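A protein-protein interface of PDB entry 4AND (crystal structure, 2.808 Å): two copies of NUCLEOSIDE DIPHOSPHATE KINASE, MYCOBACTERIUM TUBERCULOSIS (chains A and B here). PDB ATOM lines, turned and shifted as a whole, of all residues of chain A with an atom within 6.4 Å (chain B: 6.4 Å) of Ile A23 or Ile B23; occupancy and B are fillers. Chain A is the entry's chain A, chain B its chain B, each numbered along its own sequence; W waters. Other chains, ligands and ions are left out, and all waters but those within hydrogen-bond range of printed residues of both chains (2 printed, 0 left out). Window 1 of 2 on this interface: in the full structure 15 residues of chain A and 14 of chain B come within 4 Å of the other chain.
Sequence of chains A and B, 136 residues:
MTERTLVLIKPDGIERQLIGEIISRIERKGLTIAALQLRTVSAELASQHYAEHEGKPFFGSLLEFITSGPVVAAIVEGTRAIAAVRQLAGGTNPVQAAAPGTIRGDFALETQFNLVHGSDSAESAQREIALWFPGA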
ATOM      1  N   ILE A   9     -13.273 -14.956   4.097  1.00  0.00           N
ATOM      2  CA  ILE A   9     -14.629 -15.346   4.445  1.00  0.00           C
ATOM      3  C   ILE A   9     -14.904 -14.770   5.824  1.00  0.00           C
ATOM      4  O   ILE A   9     -14.435 -15.291   6.838  1.00  0.00           O
ATOM      5  CB  ILE A   9     -14.813 -16.868   4.454  1.00  0.00           C
ATOM      6  CG1 ILE A   9     -14.426 -17.452   3.095  1.00  0.00           C
ATOM      7  CG2 ILE A   9     -16.252 -17.224   4.788  1.00  0.00           C
ATOM      8  CD1 ILE A   9     -14.542 -18.953   3.023  1.00  0.00           C
ATOM      9  N   LEU A  18     -20.931 -21.315   5.394  1.00  0.00           N
ATOM     10  CA  LEU A  18     -20.721 -21.148   3.961  1.00  0.00           C
ATOM     11  C   LEU A  18     -19.251 -21.247   3.565  1.00  0.00           C
ATOM     12  O   LEU A  18     -18.889 -20.960   2.425  1.00  0.00           O
ATOM     13  CB  LEU A  18     -21.303 -19.815   3.489  1.00  0.00           C
ATOM     14  CG  LEU A  18     -22.832 -19.754   3.434  1.00  0.00           C
ATOM     15  CD1 LEU A  18     -23.323 -18.319   3.358  1.00  0.00           C
ATOM     16  CD2 LEU A  18     -23.369 -20.577   2.267  1.00  0.00           C
ATOM     17  N   ILE A  19     -18.402 -21.650   4.502  1.00  0.00           N
ATOM     18  CA  ILE A  19     -16.991 -21.818   4.192  1.00  0.00           C
ATOM     19  C   ILE A  19     -16.855 -22.783   3.021  1.00  0.00           C
ATOM     20  O   ILE A  19     -16.294 -22.432   1.976  1.00  0.00           O
ATOM     21  CB  ILE A  19     -16.205 -22.363   5.390  1.00  0.00           C
ATOM     22  CG1 ILE A  19     -16.283 -21.390   6.569  1.00  0.00           C
ATOM     23  CG2 ILE A  19     -14.762 -22.626   4.990  1.00  0.00           C
ATOM     24  CD1 ILE A  19     -15.674 -21.925   7.843  1.00  0.00           C
ATOM     25  N   GLY A  20     -17.378 -23.996   3.198  1.00  0.00           N
ATOM     26  CA  GLY A  20     -17.323 -25.011   2.165  1.00  0.00           C
ATOM     27  C   GLY A  20     -17.900 -24.499   0.861  1.00  0.00           C
ATOM     28  O   GLY A  20     -17.278 -24.617  -0.197  1.00  0.00           O
ATOM     29  N   GLU A  21     -19.093 -23.921   0.938  1.00  0.00           N
ATOM     30  CA  GLU A  21     -19.773 -23.414  -0.245  1.00  0.00           C
ATOM     31  C   GLU A  21     -18.907 -22.446  -1.053  1.00  0.00           C
ATOM     32  O   GLU A  21     -18.790 -22.569  -2.271  1.00  0.00           O
ATOM     33  CB  GLU A  21     -21.082 -22.732   0.147  1.00  0.00           C
ATOM     34  CG  GLU A  21     -21.885 -22.249  -1.044  1.00  0.00           C
ATOM     35  CD  GLU A  21     -22.375 -23.389  -1.905  1.00  0.00           C
ATOM     36  OE1 GLU A  21     -22.709 -24.452  -1.336  1.00  0.00           O
ATOM     37  OE2 GLU A  21     -22.426 -23.224  -3.145  1.00  0.00           O
ATOM     38  N   ILE A  22     -18.311 -21.477  -0.371  1.00  0.00           N
ATOM     39  CA  ILE A  22     -17.511 -20.459  -1.036  1.00  0.00           C
ATOM     40  C   ILE A  22     -16.253 -21.051  -1.676  1.00  0.00           C
ATOM     41  O   ILE A  22     -15.923 -20.746  -2.832  1.00  0.00           O
ATOM     42  CB  ILE A  22     -17.141 -19.335  -0.063  1.00  0.00           C
ATOM     43  CG1 ILE A  22     -18.391 -18.530   0.289  1.00  0.00           C
ATOM     44  CG2 ILE A  22     -16.073 -18.439  -0.662  1.00  0.00           C
ATOM     45  CD1 ILE A  22     -18.239 -17.670   1.514  1.00  0.00           C
ATOM     46  N   ILE A  23     -15.555 -21.906  -0.936  1.00  0.00           N
ATOM     47  CA  ILE A  23     -14.379 -22.562  -1.487  1.00  0.00           C
ATOM     48  C   ILE A  23     -14.750 -23.374  -2.736  1.00  0.00           C
ATOM     49  O   ILE A  23     -14.083 -23.274  -3.773  1.00  0.00           O
ATOM     50  CB  ILE A  23     -13.678 -23.438  -0.432  1.00  0.00           C
ATOM     51  CG1 ILE A  23     -13.220 -22.566   0.742  1.00  0.00           C
ATOM     52  CG2 ILE A  23     -12.501 -24.185  -1.053  1.00  0.00           C
ATOM     53  CD1 ILE A  23     -12.503 -23.323   1.832  1.00  0.00           C
ATOM     54  N   SER A  24     -15.828 -24.150  -2.642  1.00  0.00           N
ATOM     55  CA  SER A  24     -16.303 -24.944  -3.778  1.00  0.00           C
ATOM     56  C   SER A  24     -16.448 -24.098  -5.037  1.00  0.00           C
ATOM     57  O   SER A  24     -15.986 -24.482  -6.115  1.00  0.00           O
ATOM     58  CB  SER A  24     -17.643 -25.614  -3.467  1.00  0.00           C
ATOM     59  OG  SER A  24     -17.499 -26.704  -2.575  1.00  0.00           O
ATOM     60  N   ARG A  25     -17.093 -22.944  -4.903  1.00  0.00           N
ATOM     61  CA  ARG A  25     -17.325 -22.075  -6.053  1.00  0.00           C
ATOM     62  C   ARG A  25     -16.015 -21.598  -6.672  1.00  0.00           C
ATOM     63  O   ARG A  25     -15.895 -21.498  -7.900  1.00  0.00           O
ATOM     64  CB  ARG A  25     -18.227 -20.901  -5.678  1.00  0.00           C
ATOM     65  CG  ARG A  25     -19.664 -21.333  -5.424  1.00  0.00           C
ATOM     66  CD  ARG A  25     -20.555 -20.171  -5.025  1.00  0.00           C
ATOM     67  NE  ARG A  25     -21.912 -20.618  -4.721  1.00  0.00           N
ATOM     68  CZ  ARG A  25     -23.011 -19.953  -5.058  1.00  0.00           C
ATOM     69  NH1 ARG A  25     -22.924 -18.803  -5.710  1.00  0.00           N
ATOM     70  NH2 ARG A  25     -24.199 -20.443  -4.743  1.00  0.00           N
ATOM     71  N   ILE A  26     -15.027 -21.325  -5.827  1.00  0.00           N
ATOM     72  CA  ILE A  26     -13.712 -20.929  -6.314  1.00  0.00           C
ATOM     73  C   ILE A  26     -13.017 -22.081  -7.050  1.00  0.00           C
ATOM     74  O   ILE A  26     -12.516 -21.907  -8.167  1.00  0.00           O
ATOM     75  CB  ILE A  26     -12.825 -20.433  -5.165  1.00  0.00           C
ATOM     76  CG1 ILE A  26     -13.425 -19.161  -4.552  1.00  0.00           C
ATOM     77  CG2 ILE A  26     -11.395 -20.203  -5.657  1.00  0.00           C
ATOM     78  CD1 ILE A  26     -12.832 -18.782  -3.215  1.00  0.00           C
ATOM     79  N   GLU A  27     -13.000 -23.256  -6.421  1.00  0.00           N
ATOM     80  CA  GLU A  27     -12.408 -24.452  -7.024  1.00  0.00           C
ATOM     81  C   GLU A  27     -13.021 -24.783  -8.387  1.00  0.00           C
ATOM     82  O   GLU A  27     -12.310 -25.121  -9.334  1.00  0.00           O
ATOM     83  CB  GLU A  27     -12.565 -25.660  -6.090  1.00  0.00           C
ATOM     84  CG  GLU A  27     -11.531 -25.766  -4.974  1.00  0.00           C
ATOM     85  CD  GLU A  27     -11.897 -26.828  -3.948  1.00  0.00           C
ATOM     86  OE1 GLU A  27     -12.936 -26.668  -3.272  1.00  0.00           O
ATOM     87  OE2 GLU A  27     -11.155 -27.824  -3.820  1.00  0.00           O
ATOM     88  N   ARG A  28     -14.343 -24.686  -8.478  1.00  0.00           N
ATOM     89  CA  ARG A  28     -15.064 -25.076  -9.685  1.00  0.00           C
ATOM     90  C   ARG A  28     -14.889 -24.093 -10.835  1.00  0.00           C
ATOM     91  O   ARG A  28     -15.025 -24.460 -11.998  1.00  0.00           O
ATOM     92  CB  ARG A  28     -16.546 -25.309  -9.374  1.00  0.00           C
ATOM     93  CG  ARG A  28     -16.824 -26.729  -8.929  1.00  0.00           C
ATOM     94  CD  ARG A  28     -17.887 -26.813  -7.851  1.00  0.00           C
ATOM     95  NE  ARG A  28     -17.792 -28.080  -7.126  1.00  0.00           N
ATOM     96  CZ  ARG A  28     -18.663 -28.483  -6.207  1.00  0.00           C
ATOM     97  NH1 ARG A  28     -19.707 -27.718  -5.900  1.00  0.00           N
ATOM     98  NH2 ARG A  28     -18.493 -29.653  -5.598  1.00  0.00           N
ATOM     99  N   ILE A  33      -6.633 -23.056  -4.428  1.00  0.00           N
ATOM    100  CA  ILE A  33      -6.349 -22.514  -3.109  1.00  0.00           C
ATOM    101  C   ILE A  33      -4.857 -22.651  -2.823  1.00  0.00           C
ATOM    102  O   ILE A  33      -4.376 -23.741  -2.510  1.00  0.00           O
ATOM    103  CB  ILE A  33      -7.143 -23.253  -2.010  1.00  0.00           C
ATOM    104  CG1 ILE A  33      -8.592 -23.474  -2.446  1.00  0.00           C
ATOM    105  CG2 ILE A  33      -7.102 -22.474  -0.696  1.00  0.00           C
ATOM    106  CD1 ILE A  33      -9.403 -22.191  -2.527  1.00  0.00           C
ATOM    107  N   LEU A  36      -4.503 -21.143   2.847  1.00  0.00           N
ATOM    108  CA  LEU A  36      -5.791 -21.224   3.525  1.00  0.00           C
ATOM    109  C   LEU A  36      -5.621 -21.359   5.034  1.00  0.00           C
ATOM    110  O   LEU A  36      -4.928 -22.259   5.512  1.00  0.00           O
ATOM    111  CB  LEU A  36      -6.594 -22.410   2.991  1.00  0.00           C
ATOM    112  CG  LEU A  36      -7.972 -22.626   3.618  1.00  0.00           C
ATOM    113  CD1 LEU A  36      -8.928 -21.507   3.222  1.00  0.00           C
ATOM    114  CD2 LEU A  36      -8.526 -23.979   3.208  1.00  0.00           C
ATOM    115  N   VAL A  72     -11.732 -16.721   7.698  1.00  0.00           N
ATOM    116  CA  VAL A  72     -10.935 -17.623   6.882  1.00  0.00           C
ATOM    117  C   VAL A  72     -10.228 -16.815   5.810  1.00  0.00           C
ATOM    118  O   VAL A  72     -10.866 -16.242   4.930  1.00  0.00           O
ATOM    119  CB  VAL A  72     -11.779 -18.735   6.236  1.00  0.00           C
ATOM    120  CG1 VAL A  72     -10.914 -19.602   5.338  1.00  0.00           C
ATOM    121  CG2 VAL A  72     -12.434 -19.588   7.304  1.00  0.00           C
ATOM    122  N   ILE B   9      -7.760 -33.360   4.526  1.00  0.00           N
ATOM    123  CA  ILE B   9      -8.123 -33.504   3.126  1.00  0.00           C
ATOM    124  C   ILE B   9      -6.824 -33.726   2.370  1.00  0.00           C
ATOM    125  O   ILE B   9      -6.058 -32.794   2.126  1.00  0.00           O
ATOM    126  CB  ILE B   9      -8.864 -32.269   2.585  1.00  0.00           C
ATOM    127  CG1 ILE B   9     -10.047 -31.925   3.489  1.00  0.00           C
ATOM    128  CG2 ILE B   9      -9.351 -32.509   1.161  1.00  0.00           C
ATOM    129  CD1 ILE B   9     -10.781 -30.667   3.073  1.00  0.00           C
ATOM    130  N   LEU B  18     -12.196 -30.827  -4.123  1.00  0.00           N
ATOM    131  CA  LEU B  18     -13.231 -31.268  -3.196  1.00  0.00           C
ATOM    132  C   LEU B  18     -13.077 -30.660  -1.804  1.00  0.00           C
ATOM    133  O   LEU B  18     -13.758 -31.070  -0.864  1.00  0.00           O
ATOM    134  CB  LEU B  18     -13.243 -32.798  -3.097  1.00  0.00           C
ATOM    135  CG  LEU B  18     -13.709 -33.598  -4.321  1.00  0.00           C
ATOM    136  CD1 LEU B  18     -13.359 -35.072  -4.174  1.00  0.00           C
ATOM    137  CD2 LEU B  18     -15.204 -33.421  -4.565  1.00  0.00           C
ATOM    138  N   ILE B  19     -12.189 -29.684  -1.665  1.00  0.00           N
ATOM    139  CA  ILE B  19     -12.021 -29.020  -0.379  1.00  0.00           C
ATOM    140  C   ILE B  19     -13.366 -28.461   0.070  1.00  0.00           C
ATOM    141  O   ILE B  19     -13.886 -28.835   1.128  1.00  0.00           O
ATOM    142  CB  ILE B  19     -10.983 -27.886  -0.453  1.00  0.00           C
ATOM    143  CG1 ILE B  19      -9.629 -28.439  -0.903  1.00  0.00           C
ATOM    144  CG2 ILE B  19     -10.864 -27.189   0.893  1.00  0.00           C
ATOM    145  CD1 ILE B  19      -8.579 -27.382  -1.118  1.00  0.00           C
ATOM    146  N   GLY B  20     -13.926 -27.577  -0.750  1.00  0.00           N
ATOM    147  CA  GLY B  20     -15.212 -26.977  -0.464  1.00  0.00           C
ATOM    148  C   GLY B  20     -16.256 -28.029  -0.164  1.00  0.00           C
ATOM    149  O   GLY B  20     -16.944 -27.953   0.856  1.00  0.00           O
ATOM    150  N   GLU B  21     -16.360 -29.020  -1.044  1.00  0.00           N
ATOM    151  CA  GLU B  21     -17.360 -30.077  -0.909  1.00  0.00           C
ATOM    152  C   GLU B  21     -17.301 -30.756   0.459  1.00  0.00           C
ATOM    153  O   GLU B  21     -18.326 -30.915   1.133  1.00  0.00           O
ATOM    154  CB  GLU B  21     -17.187 -31.118  -2.019  1.00  0.00           C
ATOM    155  CG  GLU B  21     -18.181 -32.277  -1.961  1.00  0.00           C
ATOM    156  CD  GLU B  21     -19.612 -31.849  -2.244  1.00  0.00           C
ATOM    157  OE1 GLU B  21     -19.805 -30.838  -2.955  1.00  0.00           O
ATOM    158  OE2 GLU B  21     -20.546 -32.531  -1.765  1.00  0.00           O
ATOM    159  N   ILE B  22     -16.100 -31.151   0.867  1.00  0.00           N
ATOM    160  CA  ILE B  22     -15.917 -31.862   2.124  1.00  0.00           C
ATOM    161  C   ILE B  22     -16.252 -30.992   3.335  1.00  0.00           C
ATOM    162  O   ILE B  22     -16.937 -31.432   4.264  1.00  0.00           O
ATOM    163  CB  ILE B  22     -14.494 -32.403   2.254  1.00  0.00           C
ATOM    164  CG1 ILE B  22     -14.213 -33.426   1.147  1.00  0.00           C
ATOM    165  CG2 ILE B  22     -14.302 -33.024   3.620  1.00  0.00           C
ATOM    166  CD1 ILE B  22     -12.821 -34.033   1.202  1.00  0.00           C
ATOM    167  N   ILE B  23     -15.780 -29.753   3.326  1.00  0.00           N
ATOM    168  CA  ILE B  23     -16.103 -28.832   4.412  1.00  0.00           C
ATOM    169  C   ILE B  23     -17.622 -28.633   4.519  1.00  0.00           C
ATOM    170  O   ILE B  23     -18.188 -28.709   5.616  1.00  0.00           O
ATOM    171  CB  ILE B  23     -15.378 -27.481   4.238  1.00  0.00           C
ATOM    172  CG1 ILE B  23     -13.865 -27.698   4.261  1.00  0.00           C
ATOM    173  CG2 ILE B  23     -15.794 -26.498   5.323  1.00  0.00           C
ATOM    174  CD1 ILE B  23     -13.073 -26.502   3.802  1.00  0.00           C
ATOM    175  N   SER B  24     -18.274 -28.400   3.377  1.00  0.00           N
ATOM    176  CA  SER B  24     -19.728 -28.233   3.337  1.00  0.00           C
ATOM    177  C   SER B  24     -20.451 -29.370   4.049  1.00  0.00           C
ATOM    178  O   SER B  24     -21.326 -29.134   4.883  1.00  0.00           O
ATOM    179  CB  SER B  24     -20.226 -28.126   1.896  1.00  0.00           C
ATOM    180  OG  SER B  24     -19.845 -26.891   1.316  1.00  0.00           O
ATOM    181  N   ARG B  25     -20.080 -30.605   3.720  1.00  0.00           N
ATOM    182  CA  ARG B  25     -20.718 -31.774   4.324  1.00  0.00           C
ATOM    183  C   ARG B  25     -20.553 -31.780   5.842  1.00  0.00           C
ATOM    184  O   ARG B  25     -21.477 -32.143   6.573  1.00  0.00           O
ATOM    185  CB  ARG B  25     -20.180 -33.071   3.717  1.00  0.00           C
ATOM    186  CG  ARG B  25     -20.431 -33.203   2.229  1.00  0.00           C
ATOM    187  CD  ARG B  25     -20.047 -34.582   1.711  1.00  0.00           C
ATOM    188  NE  ARG B  25     -20.547 -34.805   0.356  1.00  0.00           N
ATOM    189  CZ  ARG B  25     -20.960 -35.980  -0.104  1.00  0.00           C
ATOM    190  NH1 ARG B  25     -20.932 -37.048   0.679  1.00  0.00           N
ATOM    191  NH2 ARG B  25     -21.401 -36.086  -1.347  1.00  0.00           N
ATOM    192  N   ILE B  26     -19.383 -31.368   6.315  1.00  0.00           N
ATOM    193  CA  ILE B  26     -19.147 -31.280   7.749  1.00  0.00           C
ATOM    194  C   ILE B  26     -20.015 -30.194   8.386  1.00  0.00           C
ATOM    195  O   ILE B  26     -20.689 -30.438   9.390  1.00  0.00           O
ATOM    196  CB  ILE B  26     -17.669 -31.018   8.056  1.00  0.00           C
ATOM    197  CG1 ILE B  26     -16.819 -32.187   7.558  1.00  0.00           C
ATOM    198  CG2 ILE B  26     -17.462 -30.818   9.549  1.00  0.00           C
ATOM    199  CD1 ILE B  26     -15.334 -31.925   7.626  1.00  0.00           C
ATOM    200  N   GLU B  27     -20.005 -29.003   7.793  1.00  0.00           N
ATOM    201  CA  GLU B  27     -20.820 -27.885   8.273  1.00  0.00           C
ATOM    202  C   GLU B  27     -22.307 -28.229   8.351  1.00  0.00           C
ATOM    203  O   GLU B  27     -22.988 -27.878   9.317  1.00  0.00           O
ATOM    204  CB  GLU B  27     -20.622 -26.653   7.381  1.00  0.00           C
ATOM    205  CG  GLU B  27     -19.248 -26.016   7.479  1.00  0.00           C
ATOM    206  CD  GLU B  27     -19.032 -24.938   6.433  1.00  0.00           C
ATOM    207  OE1 GLU B  27     -18.841 -25.285   5.248  1.00  0.00           O
ATOM    208  OE2 GLU B  27     -19.051 -23.745   6.797  1.00  0.00           O
ATOM    209  N   ARG B  28     -22.803 -28.912   7.327  1.00  0.00           N
ATOM    210  CA  ARG B  28     -24.224 -29.217   7.228  1.00  0.00           C
ATOM    211  C   ARG B  28     -24.675 -30.314   8.190  1.00  0.00           C
ATOM    212  O   ARG B  28     -25.848 -30.379   8.561  1.00  0.00           O
ATOM    213  CB  ARG B  28     -24.586 -29.544   5.782  1.00  0.00           C
ATOM    214  CG  ARG B  28     -24.603 -28.284   4.930  1.00  0.00           C
ATOM    215  CD  ARG B  28     -24.257 -28.527   3.467  1.00  0.00           C
ATOM    216  NE  ARG B  28     -24.115 -27.253   2.764  1.00  0.00           N
ATOM    217  CZ  ARG B  28     -23.781 -27.134   1.482  1.00  0.00           C
ATOM    218  NH1 ARG B  28     -23.551 -28.224   0.751  1.00  0.00           N
ATOM    219  NH2 ARG B  28     -23.678 -25.926   0.931  1.00  0.00           N
ATOM    220  N   ILE B  33     -16.032 -25.890  12.168  1.00  0.00           N
ATOM    221  CA  ILE B  33     -14.604 -25.867  11.888  1.00  0.00           C
ATOM    222  C   ILE B  33     -13.903 -25.031  12.950  1.00  0.00           C
ATOM    223  O   ILE B  33     -13.961 -23.802  12.920  1.00  0.00           O
ATOM    224  CB  ILE B  33     -14.312 -25.256  10.502  1.00  0.00           C
ATOM    225  CG1 ILE B  33     -15.271 -25.821   9.450  1.00  0.00           C
ATOM    226  CG2 ILE B  33     -12.856 -25.481  10.109  1.00  0.00           C
ATOM    227  CD1 ILE B  33     -15.163 -27.316   9.264  1.00  0.00           C
ATOM    228  N   LEU B  36      -8.429 -24.604  10.846  1.00  0.00           N
ATOM    229  CA  LEU B  36      -8.357 -24.903   9.420  1.00  0.00           C
ATOM    230  C   LEU B  36      -7.109 -24.301   8.789  1.00  0.00           C
ATOM    231  O   LEU B  36      -6.870 -23.098   8.894  1.00  0.00           O
ATOM    232  CB  LEU B  36      -9.608 -24.378   8.708  1.00  0.00           C
ATOM    233  CG  LEU B  36      -9.682 -24.482   7.180  1.00  0.00           C
ATOM    234  CD1 LEU B  36      -9.752 -25.938   6.732  1.00  0.00           C
ATOM    235  CD2 LEU B  36     -10.870 -23.691   6.639  1.00  0.00           C
ATOM    236  N   VAL B  72      -5.023 -30.184   3.584  1.00  0.00           N
ATOM    237  CA  VAL B  72      -5.816 -29.291   4.413  1.00  0.00           C
ATOM    238  C   VAL B  72      -6.097 -29.972   5.742  1.00  0.00           C
ATOM    239  O   VAL B  72      -6.794 -30.980   5.798  1.00  0.00           O
ATOM    240  CB  VAL B  72      -7.138 -28.886   3.740  1.00  0.00           C
ATOM    241  CG1 VAL B  72      -7.933 -27.977   4.662  1.00  0.00           C
ATOM    242  CG2 VAL B  72      -6.864 -28.190   2.418  1.00  0.00           C
HETATM  243  O   HOH W   1     -15.117 -28.239  -3.777  1.00  0.00           O
HETATM  244  O   HOH W   2     -20.919 -24.500   3.441  1.00  0.00           O
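Of the 15 printed residues of chain A, 9 touch a printed residue of chain B. Printed residues of chain A that touch a printed residue of chain B: Leu A18, Ile A19, Gly A20, Glu A21, Ile A23, Ser A24, Glu A27, Arg A28 and Leu A36. Among the printed residues, Asp or Glu carboxylates within 4 Å of a Lys or Arg side-chain nitrogen of the other chain: Glu A21 with Arg B28 (2.9 Å) and Arg A28 with Glu B21 (3.2 Å).
The backbone carbonyl oxygen (O) of Gly A20 sits at hydrogen-bond distance from the side-chain hydroxyl (OG) of Ser A24 (3.2 Å). NE of Arg A25 lies within salt-bridge range of OE2 of Glu A21 (3.1 Å). The backbone carbonyl oxygen (O) of Gly B20 is in hydrogen-bond range of the side-chain hydroxyl (OG) of Ser B24 (3.1 Å). The guanidinium group of Arg B25 is in salt-bridge range of the side-chain carboxylate of Glu B21 (3.1 Å).
Water W1 lies within hydrogen-bond range of the side-chain carboxylate (OE1) of Glu A27, the side-chain hydroxyl (OG) of Ser A24, the backbone NH (N) of Glu B21 and the backbone NH (N) of Gly B20. Water W2 lies within hydrogen-bond range of the side-chain carboxylate (OE1) of Glu B27, the backbone NH (N) of Glu A21 and the side-chain hydroxyl (OG) of Ser B24.
Ile A19 touches Glu B27, and with the chains exchanged Glu A27 touches Ile B19. Gly A20 touches its own counterpart, Gly B20. Gly A20 touches Ile B23, and with the chains exchanged Ile A23 touches Gly B20. Gly A20 touches Glu B27, and with the chains exchanged Glu A27 touches Gly B20. Positions printed for both chains: 9, 18, 19, 20, 21, 22, 23, 24, 25, 26, 27, 28, 33, 36 and 72. Of the 18 pairs that touch across the chains among the printed residues, 17 have their exchanged pair printed and touching as well.
Of the printed residues of chain B, Glu A21 touches Ser B24 and Arg B28. Ile A23 touches just these residues of chain B: Ile B19, Gly B20 and Ile B23. Of the printed residues of chain A, Ile B19 touches Ile A23 (3.9 Å) and Glu A27 (3.0 Å). Ile B22 touches none of the printed residues of chain A. Ile B23 touches just these residues of chain A: Gly A20 (3.6 Å) and Ile A23 (3.8 Å). The nearest residue of chain A that does not touch Ile B23 is Ile A19 (4.02 Å).
The side-chain carboxylate (OE2) of Glu B27 is in hydrogen-bond range of the backbone NH (N) of Leu A18, at 3.4 Å. The backbone NH (N) of Ile A19 sits at hydrogen-bond distance from the side-chain carboxylate (OE2) of Glu B27 (3.2 Å). N of Gly A20 sits at hydrogen-bond distance from OE1 of Glu B27, 2.8 Å away. N of Glu A21 sits at hydrogen-bond distance from OG of Ser B24 (3.1 Å). The side-chain carboxylate of Glu A21 is in salt-bridge range of the guanidinium group of Arg B28, 2.9 Å away. OG of Ser A24 sits at hydrogen-bond distance from N of Glu B21, at 3.0 Å. The backbone NH of Leu B18 lies within hydrogen-bond range of the side-chain carboxylate of Glu A27 (3.2 Å). The side-chain carboxylate (OE2) of Glu A27 lies within hydrogen-bond range of the backbone NH (N) of Ile B19, 3.0 Å away. The side-chain carboxylate of Glu A27 is in hydrogen-bond range of the backbone NH of Gly B20 (2.9 Å). The guanidinium group (NH2) of Arg A28 is in salt-bridge range of the side-chain carboxylate (OE1) of Glu B21, 3.2 Å away.
O of Gly A20 touches CA of Gly B20, at 3.1 Å. Gly A20 touches Ile B23 (N to CG2, 3.6 Å). Ser B24 touches Gly A20 (OG to C, 3.1 Å). CG2 of Ile B19 touches CG2 of Ile A23, 3.9 Å away. Ile A23 touches Gly B20 (CG2 to N, 3.7 Å). CD1 of Ile B23 touches CD1 of Ile A23, 3.8 Å away. Ser A24 touches Gly B20 (OG to C, 3.0 Å). O of Leu B36 touches O of Leu A36, at 3.99 Å.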
